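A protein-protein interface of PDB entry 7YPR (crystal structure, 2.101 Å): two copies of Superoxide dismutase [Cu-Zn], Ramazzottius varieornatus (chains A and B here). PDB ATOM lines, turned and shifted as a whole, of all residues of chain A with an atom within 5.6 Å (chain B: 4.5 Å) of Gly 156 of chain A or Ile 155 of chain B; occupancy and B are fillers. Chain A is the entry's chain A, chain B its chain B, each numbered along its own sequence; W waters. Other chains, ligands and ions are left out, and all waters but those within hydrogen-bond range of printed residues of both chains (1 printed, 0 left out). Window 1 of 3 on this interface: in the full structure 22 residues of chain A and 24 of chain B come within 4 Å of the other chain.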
ATOM      1  N   SER A  89       5.983  -1.756   1.679  1.00  0.00           N
ATOM      2  CA  SER A  89       6.476  -2.598   0.594  1.00  0.00           C
ATOM      3  C   SER A  89       5.655  -2.365  -0.670  1.00  0.00           C
ATOM      4  O   SER A  89       4.454  -2.100  -0.604  1.00  0.00           O
ATOM      5  CB  SER A  89       6.384  -4.079   0.982  1.00  0.00           C
ATOM      6  OG  SER A  89       6.917  -4.918  -0.037  1.00  0.00           O
ATOM      7  N   GLY A  90       6.310  -2.470  -1.827  1.00  0.00           N
ATOM      8  CA  GLY A  90       5.601  -2.621  -3.091  1.00  0.00           C
ATOM      9  C   GLY A  90       5.674  -4.013  -3.682  1.00  0.00           C
ATOM     10  O   GLY A  90       5.305  -4.197  -4.852  1.00  0.00           O
ATOM     11  N   ASP A  91       6.127  -5.005  -2.920  1.00  0.00           N
ATOM     12  CA  ASP A  91       6.488  -6.323  -3.441  1.00  0.00           C
ATOM     13  C   ASP A  91       5.228  -7.174  -3.603  1.00  0.00           C
ATOM     14  O   ASP A  91       4.597  -7.568  -2.621  1.00  0.00           O
ATOM     15  CB  ASP A  91       7.501  -6.977  -2.492  1.00  0.00           C
ATOM     16  CG  ASP A  91       8.016  -8.335  -3.001  1.00  0.00           C
ATOM     17  OD1 ASP A  91       7.396  -8.944  -3.904  1.00  0.00           O
ATOM     18  OD2 ASP A  91       9.042  -8.807  -2.474  1.00  0.00           O
ATOM     19  N   VAL A 154       4.446   7.927  -2.712  1.00  0.00           N
ATOM     20  CA  VAL A 154       3.711   6.670  -2.541  1.00  0.00           C
ATOM     21  C   VAL A 154       3.748   5.788  -3.783  1.00  0.00           C
ATOM     22  O   VAL A 154       3.175   4.697  -3.766  1.00  0.00           O
ATOM     23  CB  VAL A 154       2.250   6.925  -2.117  1.00  0.00           C
ATOM     24  CG1 VAL A 154       2.216   7.694  -0.798  1.00  0.00           C
ATOM     25  CG2 VAL A 154       1.481   7.692  -3.214  1.00  0.00           C
ATOM     26  N   ILE A 155       4.379   6.230  -4.867  1.00  0.00           N
ATOM     27  CA  ILE A 155       4.404   5.415  -6.074  1.00  0.00           C
ATOM     28  C   ILE A 155       5.338   4.235  -5.864  1.00  0.00           C
ATOM     29  O   ILE A 155       6.369   4.344  -5.187  1.00  0.00           O
ATOM     30  CB  ILE A 155       4.809   6.256  -7.293  1.00  0.00           C
ATOM     31  CG1 ILE A 155       3.594   7.086  -7.717  1.00  0.00           C
ATOM     32  CG2 ILE A 155       5.343   5.351  -8.442  1.00  0.00           C
ATOM     33  CD1 ILE A 155       3.843   8.022  -8.785  1.00  0.00           C
ATOM     34  N   GLY A 156       4.947   3.082  -6.390  1.00  0.00           N
ATOM     35  CA  GLY A 156       5.749   1.903  -6.225  1.00  0.00           C
ATOM     36  C   GLY A 156       5.500   1.152  -4.937  1.00  0.00           C
ATOM     37  O   GLY A 156       6.277   0.252  -4.620  1.00  0.00           O
ATOM     38  N   ARG A 157       4.446   1.494  -4.192  1.00  0.00           N
ATOM     39  CA  ARG A 157       4.059   0.831  -2.955  1.00  0.00           C
ATOM     40  C   ARG A 157       2.683   0.192  -3.130  1.00  0.00           C
ATOM     41  O   ARG A 157       1.902   0.589  -4.000  1.00  0.00           O
ATOM     42  CB  ARG A 157       3.999   1.825  -1.776  1.00  0.00           C
ATOM     43  CG  ARG A 157       5.121   2.860  -1.727  1.00  0.00           C
ATOM     44  CD  ARG A 157       6.361   2.280  -1.079  1.00  0.00           C
ATOM     45  NE  ARG A 157       7.480   3.199  -1.224  1.00  0.00           N
ATOM     46  CZ  ARG A 157       8.690   2.983  -0.728  1.00  0.00           C
ATOM     47  NH1 ARG A 157       8.964   1.895  -0.020  1.00  0.00           N
ATOM     48  NH2 ARG A 157       9.652   3.879  -0.955  1.00  0.00           N
ATOM     49  N   ILE A 158       2.362  -0.774  -2.265  1.00  0.00           N
ATOM     50  CA  ILE A 158       1.096  -1.496  -2.365  1.00  0.00           C
ATOM     51  C   ILE A 158       0.016  -0.712  -1.623  1.00  0.00           C
ATOM     52  O   ILE A 158       0.216  -0.296  -0.475  1.00  0.00           O
ATOM     53  CB  ILE A 158       1.215  -2.922  -1.800  1.00  0.00           C
ATOM     54  CG1 ILE A 158       1.992  -3.843  -2.749  1.00  0.00           C
ATOM     55  CG2 ILE A 158      -0.186  -3.529  -1.561  1.00  0.00           C
ATOM     56  CD1 ILE A 158       2.715  -4.991  -1.990  1.00  0.00           C
ATOM     57  N   ILE A 190      -0.562  -2.158  -6.776  1.00  0.00           N
ATOM     58  CA  ILE A 190       0.594  -1.266  -6.735  1.00  0.00           C
ATOM     59  C   ILE A 190       0.212   0.108  -7.276  1.00  0.00           C
ATOM     60  O   ILE A 190      -0.422   0.224  -8.334  1.00  0.00           O
ATOM     61  CB  ILE A 190       1.765  -1.859  -7.530  1.00  0.00           C
ATOM     62  CG1 ILE A 190       2.327  -3.082  -6.801  1.00  0.00           C
ATOM     63  CG2 ILE A 190       2.857  -0.812  -7.723  1.00  0.00           C
ATOM     64  CD1 ILE A 190       3.111  -4.019  -7.738  1.00  0.00           C
ATOM     65  N   ILE A 191       0.587   1.162  -6.552  1.00  0.00           N
ATOM     66  CA  ILE A 191       0.372   2.517  -7.061  1.00  0.00           C
ATOM     67  C   ILE A 191       1.450   2.833  -8.088  1.00  0.00           C
ATOM     68  O   ILE A 191       2.644   2.775  -7.785  1.00  0.00           O
ATOM     69  CB  ILE A 191       0.381   3.559  -5.931  1.00  0.00           C
ATOM     70  CG1 ILE A 191      -0.778   3.335  -4.958  1.00  0.00           C
ATOM     71  CG2 ILE A 191       0.287   4.928  -6.545  1.00  0.00           C
ATOM     72  CD1 ILE A 191      -0.691   4.219  -3.668  1.00  0.00           C
ATOM     73  N   SER A 192       1.046   3.172  -9.311  1.00  0.00           N
ATOM     74  CA  SER A 192       2.057   3.372 -10.340  1.00  0.00           C
ATOM     75  C   SER A 192       1.621   4.478 -11.272  1.00  0.00           C
ATOM     76  O   SER A 192       0.521   5.018 -11.158  1.00  0.00           O
ATOM     77  CB  SER A 192       2.309   2.076 -11.117  1.00  0.00           C
ATOM     78  OG  SER A 192       1.076   1.569 -11.541  1.00  0.00           O
ATOM     79  N   TYR A 193       2.501   4.806 -12.212  1.00  0.00           N
ATOM     80  CA  TYR A 193       2.289   5.959 -13.065  1.00  0.00           C
ATOM     81  C   TYR A 193       1.319   5.614 -14.173  1.00  0.00           C
ATOM     82  O   TYR A 193       1.387   4.527 -14.758  1.00  0.00           O
ATOM     83  CB  TYR A 193       3.600   6.423 -13.697  1.00  0.00           C
ATOM     84  CG  TYR A 193       4.570   7.151 -12.775  1.00  0.00           C
ATOM     85  CD1 TYR A 193       4.336   8.459 -12.374  1.00  0.00           C
ATOM     86  CD2 TYR A 193       5.733   6.538 -12.351  1.00  0.00           C
ATOM     87  CE1 TYR A 193       5.256   9.151 -11.564  1.00  0.00           C
ATOM     88  CE2 TYR A 193       6.653   7.216 -11.531  1.00  0.00           C
ATOM     89  CZ  TYR A 193       6.395   8.511 -11.140  1.00  0.00           C
ATOM     90  OH  TYR A 193       7.292   9.176 -10.359  1.00  0.00           O
ATOM     91  N   ALA B  40      14.321  -3.104  -5.940  1.00  0.00           N
ATOM     92  CA  ALA B  40      13.019  -3.097  -6.575  1.00  0.00           C
ATOM     93  C   ALA B  40      12.712  -4.496  -7.088  1.00  0.00           C
ATOM     94  O   ALA B  40      13.606  -5.329  -7.250  1.00  0.00           O
ATOM     95  CB  ALA B  40      12.957  -2.075  -7.713  1.00  0.00           C
ATOM     96  N   LEU B 147      16.917   3.181 -10.313  1.00  0.00           N
ATOM     97  CA  LEU B 147      15.980   2.932  -9.228  1.00  0.00           C
ATOM     98  C   LEU B 147      15.818   4.152  -8.330  1.00  0.00           C
ATOM     99  O   LEU B 147      15.092   4.082  -7.334  1.00  0.00           O
ATOM    100  CB  LEU B 147      16.426   1.734  -8.398  1.00  0.00           C
ATOM    101  CG  LEU B 147      16.728   0.479  -9.237  1.00  0.00           C
ATOM    102  CD1 LEU B 147      17.064  -0.674  -8.326  1.00  0.00           C
ATOM    103  CD2 LEU B 147      15.513   0.132 -10.097  1.00  0.00           C
ATOM    104  N   PHE B 153      14.346   7.089 -13.989  1.00  0.00           N
ATOM    105  CA  PHE B 153      13.574   6.303 -13.027  1.00  0.00           C
ATOM    106  C   PHE B 153      12.683   5.298 -13.740  1.00  0.00           C
ATOM    107  O   PHE B 153      11.901   5.684 -14.610  1.00  0.00           O
ATOM    108  CB  PHE B 153      12.707   7.277 -12.234  1.00  0.00           C
ATOM    109  CG  PHE B 153      12.189   6.765 -10.906  1.00  0.00           C
ATOM    110  CD1 PHE B 153      12.993   6.056 -10.036  1.00  0.00           C
ATOM    111  CD2 PHE B 153      10.904   7.097 -10.498  1.00  0.00           C
ATOM    112  CE1 PHE B 153      12.521   5.660  -8.793  1.00  0.00           C
ATOM    113  CE2 PHE B 153      10.428   6.694  -9.256  1.00  0.00           C
ATOM    114  CZ  PHE B 153      11.234   5.993  -8.407  1.00  0.00           C
ATOM    115  N   VAL B 154      12.757   4.023 -13.343  1.00  0.00           N
ATOM    116  CA  VAL B 154      11.866   3.002 -13.910  1.00  0.00           C
ATOM    117  C   VAL B 154      10.808   2.503 -12.932  1.00  0.00           C
ATOM    118  O   VAL B 154       9.911   1.743 -13.342  1.00  0.00           O
ATOM    119  CB  VAL B 154      12.655   1.804 -14.477  1.00  0.00           C
ATOM    120  CG1 VAL B 154      13.640   2.285 -15.548  1.00  0.00           C
ATOM    121  CG2 VAL B 154      13.395   1.038 -13.361  1.00  0.00           C
ATOM    122  N   ILE B 155      10.854   2.899 -11.673  1.00  0.00           N
ATOM    123  CA  ILE B 155       9.851   2.374 -10.757  1.00  0.00           C
ATOM    124  C   ILE B 155       8.479   2.952 -11.099  1.00  0.00           C
ATOM    125  O   ILE B 155       8.353   4.091 -11.575  1.00  0.00           O
ATOM    126  CB  ILE B 155      10.264   2.646  -9.300  1.00  0.00           C
ATOM    127  CG1 ILE B 155      11.404   1.685  -8.938  1.00  0.00           C
ATOM    128  CG2 ILE B 155       9.090   2.459  -8.347  1.00  0.00           C
ATOM    129  CD1 ILE B 155      11.909   1.853  -7.552  1.00  0.00           C
ATOM    130  N   GLY B 156       7.440   2.140 -10.917  1.00  0.00           N
ATOM    131  CA  GLY B 156       6.126   2.618 -11.256  1.00  0.00           C
ATOM    132  C   GLY B 156       5.753   2.455 -12.713  1.00  0.00           C
ATOM    133  O   GLY B 156       4.694   2.949 -13.118  1.00  0.00           O
ATOM    134  N   ARG B 157       6.579   1.765 -13.503  1.00  0.00           N
ATOM    135  CA  ARG B 157       6.341   1.506 -14.917  1.00  0.00           C
ATOM    136  C   ARG B 157       6.188   0.007 -15.140  1.00  0.00           C
ATOM    137  O   ARG B 157       6.636  -0.809 -14.332  1.00  0.00           O
ATOM    138  CB  ARG B 157       7.491   2.027 -15.783  1.00  0.00           C
ATOM    139  CG  ARG B 157       7.915   3.431 -15.450  1.00  0.00           C
ATOM    140  CD  ARG B 157       6.958   4.497 -16.004  1.00  0.00           C
ATOM    141  NE  ARG B 157       7.333   5.803 -15.459  1.00  0.00           N
ATOM    142  CZ  ARG B 157       6.741   6.957 -15.736  1.00  0.00           C
ATOM    143  NH1 ARG B 157       5.805   7.051 -16.668  1.00  0.00           N
ATOM    144  NH2 ARG B 157       7.070   8.038 -15.028  1.00  0.00           N
ATOM    145  N   ILE B 191       7.189  -2.488 -12.016  1.00  0.00           N
ATOM    146  CA  ILE B 191       8.421  -2.388 -11.246  1.00  0.00           C
ATOM    147  C   ILE B 191       8.143  -1.535 -10.015  1.00  0.00           C
ATOM    148  O   ILE B 191       7.755  -0.372 -10.141  1.00  0.00           O
ATOM    149  CB  ILE B 191       9.546  -1.784 -12.081  1.00  0.00           C
ATOM    150  CG1 ILE B 191       9.833  -2.666 -13.298  1.00  0.00           C
ATOM    151  CG2 ILE B 191      10.786  -1.638 -11.213  1.00  0.00           C
ATOM    152  CD1 ILE B 191      10.795  -1.989 -14.300  1.00  0.00           C
ATOM    153  N   SER B 192       8.348  -2.108  -8.823  1.00  0.00           N
ATOM    154  CA  SER B 192       7.974  -1.449  -7.577  1.00  0.00           C
ATOM    155  C   SER B 192       9.043  -1.689  -6.516  1.00  0.00           C
ATOM    156  O   SER B 192       9.979  -2.467  -6.714  1.00  0.00           O
ATOM    157  CB  SER B 192       6.594  -1.934  -7.095  1.00  0.00           C
ATOM    158  OG  SER B 192       6.596  -3.336  -6.917  1.00  0.00           O
ATOM    159  N   TYR B 193       8.903  -0.987  -5.382  1.00  0.00           N
ATOM    160  CA  TYR B 193       9.880  -1.064  -4.294  1.00  0.00           C
ATOM    161  C   TYR B 193       9.757  -2.386  -3.562  1.00  0.00           C
ATOM    162  O   TYR B 193       8.656  -2.901  -3.375  1.00  0.00           O
ATOM    163  CB  TYR B 193       9.668   0.077  -3.288  1.00  0.00           C
ATOM    164  CG  TYR B 193      10.137   1.436  -3.777  1.00  0.00           C
ATOM    165  CD1 TYR B 193      11.496   1.720  -3.883  1.00  0.00           C
ATOM    166  CD2 TYR B 193       9.220   2.424  -4.160  1.00  0.00           C
ATOM    167  CE1 TYR B 193      11.940   2.966  -4.330  1.00  0.00           C
ATOM    168  CE2 TYR B 193       9.653   3.681  -4.625  1.00  0.00           C
ATOM    169  CZ  TYR B 193      11.019   3.935  -4.697  1.00  0.00           C
ATOM    170  OH  TYR B 193      11.481   5.146  -5.128  1.00  0.00           O
HETATM  171  O   HOH W   1       5.945  -6.211  -7.105  1.00  0.00           O
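Ile 155 of chain A touches Tyr 193 of chain B (O to CE2, 3.4 Å). Ile 155 of chain B touches Gly 156 of chain A (CG2 to CA, 3.997 Å). Gly 156 of chain A touches Ser 192 of chain B (O to CB, 3.3 Å). Tyr 193 of chain B touches Arg 157 of chain A. Ile 190 of chain A touches Ser 192 of chain B (CD1 to OG, 3.6 Å). Ser 192 of chain A touches Gly 156 of chain B (CB to O, 3.2 Å). Tyr 193 of chain A touches Ile 155 of chain B (CE2 to O, 3.6 Å). NH2 of Arg 157 of chain B touches CD2 of Tyr 193 of chain A (3.3 Å).
The backbone carbonyl oxygen of Gly 90 of chain A is in hydrogen-bond range of the side-chain hydroxyl of Ser 192 of chain B (2.6 Å). N of Gly 90 of chain A lies within hydrogen-bond range of O of Tyr 193 of chain B (2.8 Å). O of Tyr 193 of chain B is in hydrogen-bond range of N of Asp 91 of chain A. N of Tyr 193 of chain B is in hydrogen-bond range of O of Gly 156 of chain A. N of Tyr 193 of chain A lies within hydrogen-bond range of O of Gly 156 of chain B (3.0 Å).
Water W1 lies within hydrogen-bond range of OG of Ser 192 of chain B and O of Gly 90 of chain A.
Of the 12 printed residues of chain A, 8 touch a printed residue of chain B. Printed residues of chain A that touch a printed residue of chain B: Gly 90, Asp 91, Ile 155, Gly 156, Arg 157, Ile 190, Ser 192 and Tyr 193. Hydrophobic or aromatic side chains of chain A within 4 Å of the printed part of chain B: Ile 190 and Tyr 193. Among the printed residues, no Asp or Glu carboxylate lies within 4 Å of a Lys or Arg side-chain nitrogen of the other chain.
Of the printed residues of chain B, Gly 90 of chain A touches Ser 192 (2.6 Å) and Tyr 193 (2.8 Å). Of the printed residues of chain B, Gly 156 of chain A touches Ile 155, Ser 192 and Tyr 193. Printed residues of chain B within 4 Å of Arg 157 of chain A: Tyr 193. Of the printed residues of chain B, Ile 190 of chain A touches Ser 192. Ile 191 of chain A touches none of the printed residues of chain B. Of the printed residues of chain A, Ile 155 of chain B touches Gly 156 and Tyr 193. Printed residues of chain A within 4 Å of Ser 192 of chain B: Gly 90, Gly 156 and Ile 190. The nearest printed residue of chain B that does not touch Gly 156 of chain A is Ile 191 of chain B (5.0 Å). The nearest printed residue of chain A that does not touch Ile 155 of chain B is Ile 155 of chain A (4.5 Å).
Ile 155 of chain A touches Tyr 193 of chain B, and with the chains exchanged Tyr 193 of chain A touches Ile 155 of chain B. Gly 156 of chain A touches Ser 192 of chain B, and with the chains exchanged Ser 192 of chain A touches Gly 156 of chain B. Gly 156 of chain A touches Tyr 193 of chain B, and with the chains exchanged Tyr 193 of chain A touches Gly 156 of chain B. Arg 157 of chain A touches Tyr 193 of chain B, and with the chains exchanged Tyr 193 of chain A touches Arg 157 of chain B. Positions printed for both chains: 154, 155, 156, 157, 191, 192 and 193. Of the 13 pairs that touch across the chains among the printed residues, 8 have their exchanged pair printed and touching as well.
N of Asp 91 of chain A is in hydrogen-bond range of OG of Ser 89 of chain A, at 3.0 Å. The backbone NH (N) of Gly 156 of chain A sits at hydrogen-bond distance from the backbone carbonyl oxygen (O) of Ile 191 of chain A, at 2.7 Å. N of Ile 191 of chain A lies within hydrogen-bond range of O of Arg 157 of chain A, at 2.9 Å. O of Ile 191 of chain B is in hydrogen-bond range of N of Gly 156 of chain B. N of Ile 191 of chain B is in hydrogen-bond range of O of Arg 157 of chain B.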
